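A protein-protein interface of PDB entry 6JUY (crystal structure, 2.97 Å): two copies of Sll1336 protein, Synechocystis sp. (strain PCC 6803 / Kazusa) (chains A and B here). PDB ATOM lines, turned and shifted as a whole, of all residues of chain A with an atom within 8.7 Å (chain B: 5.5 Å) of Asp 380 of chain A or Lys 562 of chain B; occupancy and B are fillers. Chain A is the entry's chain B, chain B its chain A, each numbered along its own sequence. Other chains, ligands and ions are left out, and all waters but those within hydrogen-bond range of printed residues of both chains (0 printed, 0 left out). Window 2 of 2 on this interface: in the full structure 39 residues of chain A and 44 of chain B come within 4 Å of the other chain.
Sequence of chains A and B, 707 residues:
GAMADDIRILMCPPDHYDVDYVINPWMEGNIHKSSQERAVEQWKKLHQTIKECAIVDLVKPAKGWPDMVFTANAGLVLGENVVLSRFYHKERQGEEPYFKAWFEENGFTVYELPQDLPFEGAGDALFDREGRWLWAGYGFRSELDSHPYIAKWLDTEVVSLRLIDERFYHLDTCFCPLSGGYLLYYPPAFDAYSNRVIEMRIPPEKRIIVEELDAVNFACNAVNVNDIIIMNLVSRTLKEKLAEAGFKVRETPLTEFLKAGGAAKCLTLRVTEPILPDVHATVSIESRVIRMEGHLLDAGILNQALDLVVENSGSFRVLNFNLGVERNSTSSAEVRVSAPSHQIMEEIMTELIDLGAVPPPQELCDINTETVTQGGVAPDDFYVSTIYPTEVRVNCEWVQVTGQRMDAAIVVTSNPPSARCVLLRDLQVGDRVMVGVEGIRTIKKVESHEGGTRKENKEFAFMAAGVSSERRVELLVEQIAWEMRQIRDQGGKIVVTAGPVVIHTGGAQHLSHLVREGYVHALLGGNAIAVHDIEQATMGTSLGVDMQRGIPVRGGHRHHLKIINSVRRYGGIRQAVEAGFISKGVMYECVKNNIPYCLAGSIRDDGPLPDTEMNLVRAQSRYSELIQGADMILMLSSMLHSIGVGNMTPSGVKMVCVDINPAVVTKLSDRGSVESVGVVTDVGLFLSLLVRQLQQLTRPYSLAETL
OD1 of Asn 565 of chain B is in hydrogen-bond range of N of Ala 378 of chain A.
The backbone carbonyl oxygen (O) of Asp 380 of chain A sits at hydrogen-bond distance from the side-chain amino group (NZ) of Lys 562 of chain B.
The backbone carbonyl oxygen (O) of Ala 378 of chain A sits at hydrogen-bond distance from the guanidinium group (NH2) of Arg 569 of chain B.
NH2 of Arg 569 of chain B is in salt-bridge range of OD1 of Asp 380 of chain A.
His 559 of chain B touches Glu 347 of chain A.
Asn 565 of chain B touches Val 377 of chain A (OD1 to CA, 3.8 Å).
Arg 569 of chain B touches Val 377 of chain A (NE to CG1, 3.6 Å).
Lys 562 of chain B touches Phe 382 of chain A.
CE1 of Phe 382 of chain A touches ND2 of Asn 565 of chain B (3.8 Å).
Val 384 of chain A touches Arg 558 of chain B (CG2 to CB, 3.7 Å).
Val 384 of chain A touches Leu 561 of chain B (CG1 to CD1, 3.6 Å).
Asp 407 of chain A touches Leu 561 of chain B.
Asn 565 of chain B touches Leu 424 of chain A.
The backbone carbonyl oxygen (O) of Glu 347 of chain A is in hydrogen-bond range of the side-chain hydroxyl (OG1) of Thr 350 of chain A (2.8 Å).
The side-chain hydroxyl of Ser 566 of chain B sits at hydrogen-bond distance from the backbone carbonyl oxygen of Lys 562 of chain B.
The side-chain amide nitrogen (ND2) of Asn 565 of chain B lies close to the guanidinium group (NH2) of Arg 569 of chain B, 3.3 Å away.
The backbone carbonyl oxygen (O) of Ser 385 of chain A lies within hydrogen-bond range of the backbone NH (N) of Asp 407 of chain A (2.7 Å).
Glu 370 of chain A touches none of the printed residues of chain B.
Of the printed residues of chain B, Ala 378 of chain A touches Asn 565 and Arg 569.
Asp 380 of chain A touches just these residues of chain B: Lys 562 and Arg 569.
Of the printed residues of chain B, Phe 382 of chain A touches Lys 562 and Asn 565.
Of the printed residues of chain A, Lys 562 of chain B touches Asp 380 and Phe 382.
Val 567 of chain B touches none of the printed residues of chain A.
Of the printed residues of chain A, Arg 569 of chain B touches Val 377 (3.6 Å), Ala 378 (3.5 Å) and Asp 380 (2.5 Å).
The nearest printed residue of chain A that does not touch Lys 562 of chain B is Asp 381 of chain A (4.01 Å).
No position is printed for both chains.
Hydrophobic or aromatic side chains of chain A that line the printed part of chain B: Val 377, Ala 378, Phe 382, Val 384 and Leu 424.
Along chain A the printed residues that touch a printed residue of chain B span positions 347 to 424.
Hydrophobic or aromatic side chains of chain B within 4 Å of the printed part of chain A: His 559 and Leu 561.
Among the printed residues, 13 pairs touch across the chains.
Among the printed residues, Asp or Glu carboxylates within 4 Å of a Lys or Arg side-chain nitrogen of the other chain: Asp 380 of chain A with Arg 569 of chain B (2.5 Å).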
ATOM      1  N   GLN A 343      18.818 -21.333 -24.365  1.00  0.00           N
ATOM      2  CA  GLN A 343      19.050 -20.084 -23.640  1.00  0.00           C
ATOM      3  C   GLN A 343      20.279 -19.312 -24.152  1.00  0.00           C
ATOM      4  O   GLN A 343      20.965 -18.648 -23.370  1.00  0.00           O
ATOM      5  CB  GLN A 343      19.173 -20.331 -22.129  1.00  0.00           C
ATOM      6  CG  GLN A 343      17.977 -21.039 -21.437  1.00  0.00           C
ATOM      7  CD  GLN A 343      16.695 -20.204 -21.348  1.00  0.00           C
ATOM      8  OE1 GLN A 343      16.417 -19.583 -20.322  1.00  0.00           O
ATOM      9  NE2 GLN A 343      15.896 -20.220 -22.408  1.00  0.00           N
ATOM     10  N   GLU A 346      19.164 -16.081 -23.721  1.00  0.00           N
ATOM     11  CA  GLU A 346      19.507 -15.513 -22.422  1.00  0.00           C
ATOM     12  C   GLU A 346      20.671 -14.530 -22.529  1.00  0.00           C
ATOM     13  O   GLU A 346      20.582 -13.390 -22.059  1.00  0.00           O
ATOM     14  CB  GLU A 346      19.857 -16.652 -21.460  1.00  0.00           C
ATOM     15  CG  GLU A 346      19.376 -16.500 -20.045  1.00  0.00           C
ATOM     16  CD  GLU A 346      19.065 -17.827 -19.394  1.00  0.00           C
ATOM     17  OE1 GLU A 346      19.901 -18.750 -19.483  1.00  0.00           O
ATOM     18  OE2 GLU A 346      17.975 -17.948 -18.799  1.00  0.00           O
ATOM     19  N   GLU A 347      21.776 -14.958 -23.148  1.00  0.00           N
ATOM     20  CA  GLU A 347      22.948 -14.095 -23.288  1.00  0.00           C
ATOM     21  C   GLU A 347      22.635 -12.877 -24.149  1.00  0.00           C
ATOM     22  O   GLU A 347      23.003 -11.736 -23.806  1.00  0.00           O
ATOM     23  CB  GLU A 347      24.107 -14.896 -23.881  1.00  0.00           C
ATOM     24  CG  GLU A 347      24.385 -16.202 -23.154  1.00  0.00           C
ATOM     25  CD  GLU A 347      25.378 -17.080 -23.889  1.00  0.00           C
ATOM     26  OE1 GLU A 347      25.733 -16.742 -25.038  1.00  0.00           O
ATOM     27  OE2 GLU A 347      25.801 -18.107 -23.320  1.00  0.00           O
ATOM     28  N   THR A 350      20.693 -10.462 -21.995  1.00  0.00           N
ATOM     29  CA  THR A 350      21.475  -9.717 -21.005  1.00  0.00           C
ATOM     30  C   THR A 350      22.197  -8.555 -21.670  1.00  0.00           C
ATOM     31  O   THR A 350      22.123  -7.401 -21.211  1.00  0.00           O
ATOM     32  CB  THR A 350      22.501 -10.611 -20.296  1.00  0.00           C
ATOM     33  OG1 THR A 350      23.596 -10.891 -21.179  1.00  0.00           O
ATOM     34  CG2 THR A 350      21.883 -11.907 -19.814  1.00  0.00           C
ATOM     35  N   GLU A 370      16.292 -18.409  -7.526  1.00  0.00           N
ATOM     36  CA  GLU A 370      16.459 -19.766  -7.039  1.00  0.00           C
ATOM     37  C   GLU A 370      17.331 -19.712  -5.797  1.00  0.00           C
ATOM     38  O   GLU A 370      18.217 -18.861  -5.678  1.00  0.00           O
ATOM     39  CB  GLU A 370      17.070 -20.683  -8.108  1.00  0.00           C
ATOM     40  CG  GLU A 370      16.203 -20.829  -9.352  1.00  0.00           C
ATOM     41  CD  GLU A 370      16.687 -21.916 -10.288  1.00  0.00           C
ATOM     42  OE1 GLU A 370      17.610 -22.666  -9.905  1.00  0.00           O
ATOM     43  OE2 GLU A 370      16.142 -22.023 -11.408  1.00  0.00           O
ATOM     44  N   THR A 371      17.074 -20.631  -4.873  1.00  0.00           N
ATOM     45  CA  THR A 371      17.699 -20.582  -3.563  1.00  0.00           C
ATOM     46  C   THR A 371      19.064 -21.254  -3.567  1.00  0.00           C
ATOM     47  O   THR A 371      19.317 -22.201  -4.316  1.00  0.00           O
ATOM     48  CB  THR A 371      16.807 -21.239  -2.508  1.00  0.00           C
ATOM     49  OG1 THR A 371      15.748 -20.343  -2.150  1.00  0.00           O
ATOM     50  N   VAL A 377      28.126 -21.360  -3.951  1.00  0.00           N
ATOM     51  CA  VAL A 377      27.710 -21.809  -5.273  1.00  0.00           C
ATOM     52  C   VAL A 377      26.380 -21.144  -5.603  1.00  0.00           C
ATOM     53  O   VAL A 377      25.583 -20.831  -4.716  1.00  0.00           O
ATOM     54  CB  VAL A 377      27.600 -23.353  -5.342  1.00  0.00           C
ATOM     55  CG1 VAL A 377      27.349 -23.822  -6.765  1.00  0.00           C
ATOM     56  CG2 VAL A 377      28.855 -24.003  -4.790  1.00  0.00           C
ATOM     57  N   ALA A 378      26.146 -20.925  -6.892  1.00  0.00           N
ATOM     58  CA  ALA A 378      24.955 -20.279  -7.419  1.00  0.00           C
ATOM     59  C   ALA A 378      24.175 -21.229  -8.315  1.00  0.00           C
ATOM     60  O   ALA A 378      24.728 -22.215  -8.816  1.00  0.00           O
ATOM     61  CB  ALA A 378      25.319 -19.012  -8.210  1.00  0.00           C
ATOM     62  N   PRO A 379      22.879 -20.985  -8.511  1.00  0.00           N
ATOM     63  CA  PRO A 379      22.127 -21.771  -9.497  1.00  0.00           C
ATOM     64  C   PRO A 379      22.728 -21.594 -10.885  1.00  0.00           C
ATOM     65  O   PRO A 379      23.174 -20.508 -11.249  1.00  0.00           O
ATOM     66  CB  PRO A 379      20.708 -21.189  -9.426  1.00  0.00           C
ATOM     67  CG  PRO A 379      20.709 -20.163  -8.331  1.00  0.00           C
ATOM     68  CD  PRO A 379      22.005 -20.228  -7.601  1.00  0.00           C
ATOM     69  N   ASP A 380      22.736 -22.684 -11.661  1.00  0.00           N
ATOM     70  CA  ASP A 380      23.423 -22.686 -12.952  1.00  0.00           C
ATOM     71  C   ASP A 380      22.937 -21.571 -13.868  1.00  0.00           C
ATOM     72  O   ASP A 380      23.685 -21.117 -14.742  1.00  0.00           O
ATOM     73  CB  ASP A 380      23.247 -24.037 -13.646  1.00  0.00           C
ATOM     74  CG  ASP A 380      24.313 -25.034 -13.251  1.00  0.00           C
ATOM     75  OD1 ASP A 380      24.177 -25.661 -12.182  1.00  0.00           O
ATOM     76  OD2 ASP A 380      25.294 -25.180 -14.008  1.00  0.00           O
ATOM     77  N   ASP A 381      21.698 -21.117 -13.695  1.00  0.00           N
ATOM     78  CA  ASP A 381      21.117 -20.094 -14.550  1.00  0.00           C
ATOM     79  C   ASP A 381      21.125 -18.721 -13.889  1.00  0.00           C
ATOM     80  O   ASP A 381      20.352 -17.843 -14.286  1.00  0.00           O
ATOM     81  CB  ASP A 381      19.700 -20.495 -14.953  1.00  0.00           C
ATOM     82  CG  ASP A 381      19.301 -19.939 -16.302  1.00  0.00           C
ATOM     83  OD1 ASP A 381      19.598 -20.589 -17.327  1.00  0.00           O
ATOM     84  OD2 ASP A 381      18.695 -18.849 -16.335  1.00  0.00           O
ATOM     85  N   PHE A 382      21.979 -18.522 -12.884  1.00  0.00           N
ATOM     86  CA  PHE A 382      22.028 -17.243 -12.191  1.00  0.00           C
ATOM     87  C   PHE A 382      22.425 -16.128 -13.149  1.00  0.00           C
ATOM     88  O   PHE A 382      23.283 -16.304 -14.021  1.00  0.00           O
ATOM     89  CB  PHE A 382      23.011 -17.314 -11.017  1.00  0.00           C
ATOM     90  CG  PHE A 382      24.462 -17.228 -11.420  1.00  0.00           C
ATOM     91  CD1 PHE A 382      25.140 -18.349 -11.870  1.00  0.00           C
ATOM     92  CD2 PHE A 382      25.155 -16.032 -11.320  1.00  0.00           C
ATOM     93  CE1 PHE A 382      26.471 -18.279 -12.233  1.00  0.00           C
ATOM     94  CE2 PHE A 382      26.488 -15.955 -11.681  1.00  0.00           C
ATOM     95  CZ  PHE A 382      27.146 -17.080 -12.137  1.00  0.00           C
ATOM     96  N   TYR A 383      21.783 -14.976 -12.984  1.00  0.00           N
ATOM     97  CA  TYR A 383      22.087 -13.823 -13.817  1.00  0.00           C
ATOM     98  C   TYR A 383      23.429 -13.239 -13.400  1.00  0.00           C
ATOM     99  O   TYR A 383      23.691 -13.047 -12.208  1.00  0.00           O
ATOM    100  CB  TYR A 383      20.973 -12.783 -13.685  1.00  0.00           C
ATOM    101  CG  TYR A 383      21.273 -11.439 -14.312  1.00  0.00           C
ATOM    102  CD1 TYR A 383      21.078 -11.227 -15.672  1.00  0.00           C
ATOM    103  CD2 TYR A 383      21.740 -10.380 -13.545  1.00  0.00           C
ATOM    104  CE1 TYR A 383      21.344 -10.000 -16.250  1.00  0.00           C
ATOM    105  CE2 TYR A 383      22.015  -9.152 -14.115  1.00  0.00           C
ATOM    106  CZ  TYR A 383      21.811  -8.966 -15.467  1.00  0.00           C
ATOM    107  OH  TYR A 383      22.081  -7.743 -16.039  1.00  0.00           O
ATOM    108  N   VAL A 384      24.281 -12.957 -14.379  1.00  0.00           N
ATOM    109  CA  VAL A 384      25.591 -12.375 -14.115  1.00  0.00           C
ATOM    110  C   VAL A 384      25.463 -10.864 -14.244  1.00  0.00           C
ATOM    111  O   VAL A 384      25.076 -10.352 -15.300  1.00  0.00           O
ATOM    112  CB  VAL A 384      26.654 -12.929 -15.074  1.00  0.00           C
ATOM    113  CG1 VAL A 384      28.045 -12.515 -14.620  1.00  0.00           C
ATOM    114  CG2 VAL A 384      26.548 -14.445 -15.154  1.00  0.00           C
ATOM    115  N   SER A 385      25.800 -10.155 -13.171  1.00  0.00           N
ATOM    116  CA  SER A 385      25.632  -8.711 -13.139  1.00  0.00           C
ATOM    117  C   SER A 385      26.694  -8.022 -13.985  1.00  0.00           C
ATOM    118  O   SER A 385      27.795  -8.538 -14.193  1.00  0.00           O
ATOM    119  CB  SER A 385      25.686  -8.200 -11.699  1.00  0.00           C
ATOM    120  OG  SER A 385      26.924  -8.519 -11.089  1.00  0.00           O
ATOM    121  N   ASP A 407      30.092  -9.058 -12.912  1.00  0.00           N
ATOM    122  CA  ASP A 407      30.436 -10.453 -12.671  1.00  0.00           C
ATOM    123  C   ASP A 407      30.116 -10.863 -11.232  1.00  0.00           C
ATOM    124  O   ASP A 407      30.975 -11.344 -10.489  1.00  0.00           O
ATOM    125  CB  ASP A 407      31.906 -10.708 -13.013  1.00  0.00           C
ATOM    126  CG  ASP A 407      32.175 -10.620 -14.502  1.00  0.00           C
ATOM    127  OD1 ASP A 407      31.198 -10.529 -15.279  1.00  0.00           O
ATOM    128  OD2 ASP A 407      33.359 -10.611 -14.892  1.00  0.00           O
ATOM    129  N   LEU A 424      30.301 -14.681  -5.755  1.00  0.00           N
ATOM    130  CA  LEU A 424      29.987 -16.103  -5.644  1.00  0.00           C
ATOM    131  C   LEU A 424      30.457 -16.681  -4.311  1.00  0.00           C
ATOM    132  O   LEU A 424      29.724 -17.437  -3.667  1.00  0.00           O
ATOM    133  CB  LEU A 424      30.600 -16.879  -6.809  1.00  0.00           C
ATOM    134  CG  LEU A 424      30.083 -16.641  -8.230  1.00  0.00           C
ATOM    135  CD1 LEU A 424      30.719 -17.645  -9.181  1.00  0.00           C
ATOM    136  CD2 LEU A 424      28.565 -16.722  -8.298  1.00  0.00           C
ATOM    137  N   VAL A 433      18.745 -15.989  -5.342  1.00  0.00           N
ATOM    138  CA  VAL A 433      19.570 -15.350  -6.361  1.00  0.00           C
ATOM    139  C   VAL A 433      18.756 -15.205  -7.637  1.00  0.00           C
ATOM    140  O   VAL A 433      18.134 -16.171  -8.092  1.00  0.00           O
ATOM    141  CB  VAL A 433      20.849 -16.163  -6.628  1.00  0.00           C
ATOM    142  CG1 VAL A 433      21.598 -15.615  -7.835  1.00  0.00           C
ATOM    143  CG2 VAL A 433      21.740 -16.169  -5.398  1.00  0.00           C
ATOM    144  N   MET A 434      18.804 -14.016  -8.237  1.00  0.00           N
ATOM    145  CA  MET A 434      18.085 -13.786  -9.483  1.00  0.00           C
ATOM    146  C   MET A 434      18.594 -14.727 -10.566  1.00  0.00           C
ATOM    147  O   MET A 434      19.796 -14.992 -10.675  1.00  0.00           O
ATOM    148  CB  MET A 434      18.239 -12.334  -9.932  1.00  0.00           C
ATOM    149  CG  MET A 434      17.415 -11.980 -11.160  1.00  0.00           C
ATOM    150  SD  MET A 434      17.922 -10.420 -11.900  1.00  0.00           S
ATOM    151  N   VAL A 435      17.666 -15.230 -11.376  1.00  0.00           N
ATOM    152  CA  VAL A 435      17.959 -16.227 -12.393  1.00  0.00           C
ATOM    153  C   VAL A 435      17.281 -15.807 -13.687  1.00  0.00           C
ATOM    154  O   VAL A 435      16.187 -15.233 -13.680  1.00  0.00           O
ATOM    155  CB  VAL A 435      17.481 -17.625 -11.931  1.00  0.00           C
ATOM    156  CG1 VAL A 435      17.380 -18.601 -13.093  1.00  0.00           C
ATOM    157  CG2 VAL A 435      18.398 -18.170 -10.846  1.00  0.00           C
ATOM    158  N   GLY A 436      17.934 -16.102 -14.809  1.00  0.00           N
ATOM    159  CA  GLY A 436      17.353 -15.747 -16.082  1.00  0.00           C
ATOM    160  C   GLY A 436      17.520 -14.278 -16.425  1.00  0.00           C
ATOM    161  O   GLY A 436      18.404 -13.568 -15.932  1.00  0.00           O
ATOM    162  N   VAL A 437      16.636 -13.828 -17.311  1.00  0.00           N
ATOM    163  CA  VAL A 437      16.654 -12.481 -17.857  1.00  0.00           C
ATOM    164  C   VAL A 437      15.381 -11.712 -17.527  1.00  0.00           C
ATOM    165  O   VAL A 437      15.251 -10.546 -17.912  1.00  0.00           O
ATOM    166  CB  VAL A 437      16.878 -12.533 -19.384  1.00  0.00           C
ATOM    167  CG1 VAL A 437      17.199 -11.198 -19.936  1.00  0.00           C
ATOM    168  CG2 VAL A 437      18.012 -13.462 -19.708  1.00  0.00           C
ATOM    169  N   ARG B 558      30.173 -13.743 -19.149  1.00  0.00           N
ATOM    170  CA  ARG B 558      29.435 -14.596 -18.230  1.00  0.00           C
ATOM    171  C   ARG B 558      29.938 -16.027 -18.275  1.00  0.00           C
ATOM    172  O   ARG B 558      29.808 -16.749 -17.279  1.00  0.00           O
ATOM    173  CB  ARG B 558      27.940 -14.566 -18.561  1.00  0.00           C
ATOM    174  N   HIS B 559      30.499 -16.450 -19.413  1.00  0.00           N
ATOM    175  CA  HIS B 559      31.059 -17.792 -19.506  1.00  0.00           C
ATOM    176  C   HIS B 559      32.114 -18.013 -18.430  1.00  0.00           C
ATOM    177  O   HIS B 559      32.194 -19.099 -17.843  1.00  0.00           O
ATOM    178  CB  HIS B 559      31.652 -18.010 -20.898  1.00  0.00           C
ATOM    179  CG  HIS B 559      30.629 -18.056 -21.991  1.00  0.00           C
ATOM    180  ND1 HIS B 559      29.910 -16.949 -22.386  1.00  0.00           N
ATOM    181  CD2 HIS B 559      30.236 -19.067 -22.802  1.00  0.00           C
ATOM    182  CE1 HIS B 559      29.099 -17.282 -23.374  1.00  0.00           C
ATOM    183  NE2 HIS B 559      29.279 -18.561 -23.648  1.00  0.00           N
ATOM    184  N   HIS B 560      32.916 -16.981 -18.143  1.00  0.00           N
ATOM    185  CA  HIS B 560      33.913 -17.085 -17.080  1.00  0.00           C
ATOM    186  C   HIS B 560      33.266 -17.464 -15.755  1.00  0.00           C
ATOM    187  O   HIS B 560      33.665 -18.443 -15.115  1.00  0.00           O
ATOM    188  CB  HIS B 560      34.676 -15.767 -16.916  1.00  0.00           C
ATOM    189  CG  HIS B 560      35.548 -15.401 -18.075  1.00  0.00           C
ATOM    190  ND1 HIS B 560      35.165 -15.582 -19.384  1.00  0.00           N
ATOM    191  CD2 HIS B 560      36.776 -14.829 -18.116  1.00  0.00           C
ATOM    192  CE1 HIS B 560      36.124 -15.151 -20.183  1.00  0.00           C
ATOM    193  NE2 HIS B 560      37.112 -14.687 -19.439  1.00  0.00           N
ATOM    194  N   LEU B 561      32.258 -16.699 -15.322  1.00  0.00           N
ATOM    195  CA  LEU B 561      31.639 -17.001 -14.034  1.00  0.00           C
ATOM    196  C   LEU B 561      30.892 -18.317 -14.042  1.00  0.00           C
ATOM    197  O   LEU B 561      30.871 -19.009 -13.029  1.00  0.00           O
ATOM    198  CB  LEU B 561      30.703 -15.896 -13.572  1.00  0.00           C
ATOM    199  CG  LEU B 561      31.375 -14.700 -12.929  1.00  0.00           C
ATOM    200  CD1 LEU B 561      30.293 -13.928 -12.234  1.00  0.00           C
ATOM    201  CD2 LEU B 561      32.415 -15.202 -11.914  1.00  0.00           C
ATOM    202  N   LYS B 562      30.200 -18.645 -15.127  1.00  0.00           N
ATOM    203  CA  LYS B 562      29.511 -19.930 -15.161  1.00  0.00           C
ATOM    204  C   LYS B 562      30.495 -21.084 -15.000  1.00  0.00           C
ATOM    205  O   LYS B 562      30.246 -22.020 -14.227  1.00  0.00           O
ATOM    206  CB  LYS B 562      28.693 -20.052 -16.445  1.00  0.00           C
ATOM    207  CG  LYS B 562      27.721 -18.889 -16.634  1.00  0.00           C
ATOM    208  CD  LYS B 562      26.260 -19.310 -16.615  1.00  0.00           C
ATOM    209  CE  LYS B 562      25.361 -18.097 -16.395  1.00  0.00           C
ATOM    210  NZ  LYS B 562      23.944 -18.346 -16.786  1.00  0.00           N
ATOM    211  N   ILE B 563      31.631 -21.023 -15.703  1.00  0.00           N
ATOM    212  CA  ILE B 563      32.645 -22.067 -15.573  1.00  0.00           C
ATOM    213  C   ILE B 563      33.176 -22.113 -14.145  1.00  0.00           C
ATOM    214  O   ILE B 563      33.280 -23.185 -13.529  1.00  0.00           O
ATOM    215  CB  ILE B 563      33.780 -21.831 -16.586  1.00  0.00           C
ATOM    216  CG1 ILE B 563      33.291 -22.080 -18.014  1.00  0.00           C
ATOM    217  CG2 ILE B 563      34.979 -22.704 -16.258  1.00  0.00           C
ATOM    218  CD1 ILE B 563      33.001 -23.528 -18.317  1.00  0.00           C
ATOM    219  N   ILE B 564      33.521 -20.943 -13.602  1.00  0.00           N
ATOM    220  CA  ILE B 564      34.031 -20.858 -12.237  1.00  0.00           C
ATOM    221  C   ILE B 564      33.008 -21.405 -11.250  1.00  0.00           C
ATOM    222  O   ILE B 564      33.356 -22.107 -10.296  1.00  0.00           O
ATOM    223  CB  ILE B 564      34.416 -19.405 -11.909  1.00  0.00           C
ATOM    224  CG1 ILE B 564      35.668 -18.994 -12.681  1.00  0.00           C
ATOM    225  CG2 ILE B 564      34.666 -19.250 -10.433  1.00  0.00           C
ATOM    226  CD1 ILE B 564      35.997 -17.525 -12.553  1.00  0.00           C
ATOM    227  N   ASN B 565      31.734 -21.070 -11.456  1.00  0.00           N
ATOM    228  CA  ASN B 565      30.660 -21.511 -10.576  1.00  0.00           C
ATOM    229  C   ASN B 565      30.537 -23.025 -10.580  1.00  0.00           C
ATOM    230  O   ASN B 565      30.406 -23.651  -9.523  1.00  0.00           O
ATOM    231  CB  ASN B 565      29.348 -20.860 -11.015  1.00  0.00           C
ATOM    232  CG  ASN B 565      28.220 -21.106 -10.041  1.00  0.00           C
ATOM    233  OD1 ASN B 565      28.351 -20.854  -8.844  1.00  0.00           O
ATOM    234  ND2 ASN B 565      27.097 -21.597 -10.551  1.00  0.00           N
ATOM    235  N   SER B 566      30.545 -23.632 -11.768  1.00  0.00           N
ATOM    236  CA  SER B 566      30.516 -25.090 -11.842  1.00  0.00           C
ATOM    237  C   SER B 566      31.697 -25.696 -11.090  1.00  0.00           C
ATOM    238  O   SER B 566      31.526 -26.583 -10.239  1.00  0.00           O
ATOM    239  CB  SER B 566      30.514 -25.541 -13.302  1.00  0.00           C
ATOM    240  OG  SER B 566      29.383 -25.036 -13.988  1.00  0.00           O
ATOM    241  N   VAL B 567      32.902 -25.184 -11.350  1.00  0.00           N
ATOM    242  CA  VAL B 567      34.089 -25.767 -10.727  1.00  0.00           C
ATOM    243  C   VAL B 567      34.030 -25.610  -9.213  1.00  0.00           C
ATOM    244  O   VAL B 567      34.441 -26.507  -8.467  1.00  0.00           O
ATOM    245  CB  VAL B 567      35.363 -25.145 -11.326  1.00  0.00           C
ATOM    246  CG1 VAL B 567      36.596 -25.721 -10.656  1.00  0.00           C
ATOM    247  CG2 VAL B 567      35.411 -25.405 -12.821  1.00  0.00           C
ATOM    248  N   ARG B 569      31.240 -25.592  -7.569  1.00  0.00           N
ATOM    249  CA  ARG B 569      30.256 -26.584  -7.144  1.00  0.00           C
ATOM    250  C   ARG B 569      30.928 -27.916  -6.863  1.00  0.00           C
ATOM    251  O   ARG B 569      30.668 -28.554  -5.836  1.00  0.00           O
ATOM    252  CB  ARG B 569      29.172 -26.784  -8.203  1.00  0.00           C
ATOM    253  CG  ARG B 569      27.950 -27.501  -7.646  1.00  0.00           C
ATOM    254  CD  ARG B 569      26.828 -27.646  -8.655  1.00  0.00           C
ATOM    255  NE  ARG B 569      26.341 -26.367  -9.153  1.00  0.00           N
ATOM    256  CZ  ARG B 569      26.561 -25.919 -10.383  1.00  0.00           C
ATOM    257  NH1 ARG B 569      27.256 -26.653 -11.242  1.00  0.00           N
ATOM    258  NH2 ARG B 569      26.080 -24.741 -10.756  1.00  0.00           N
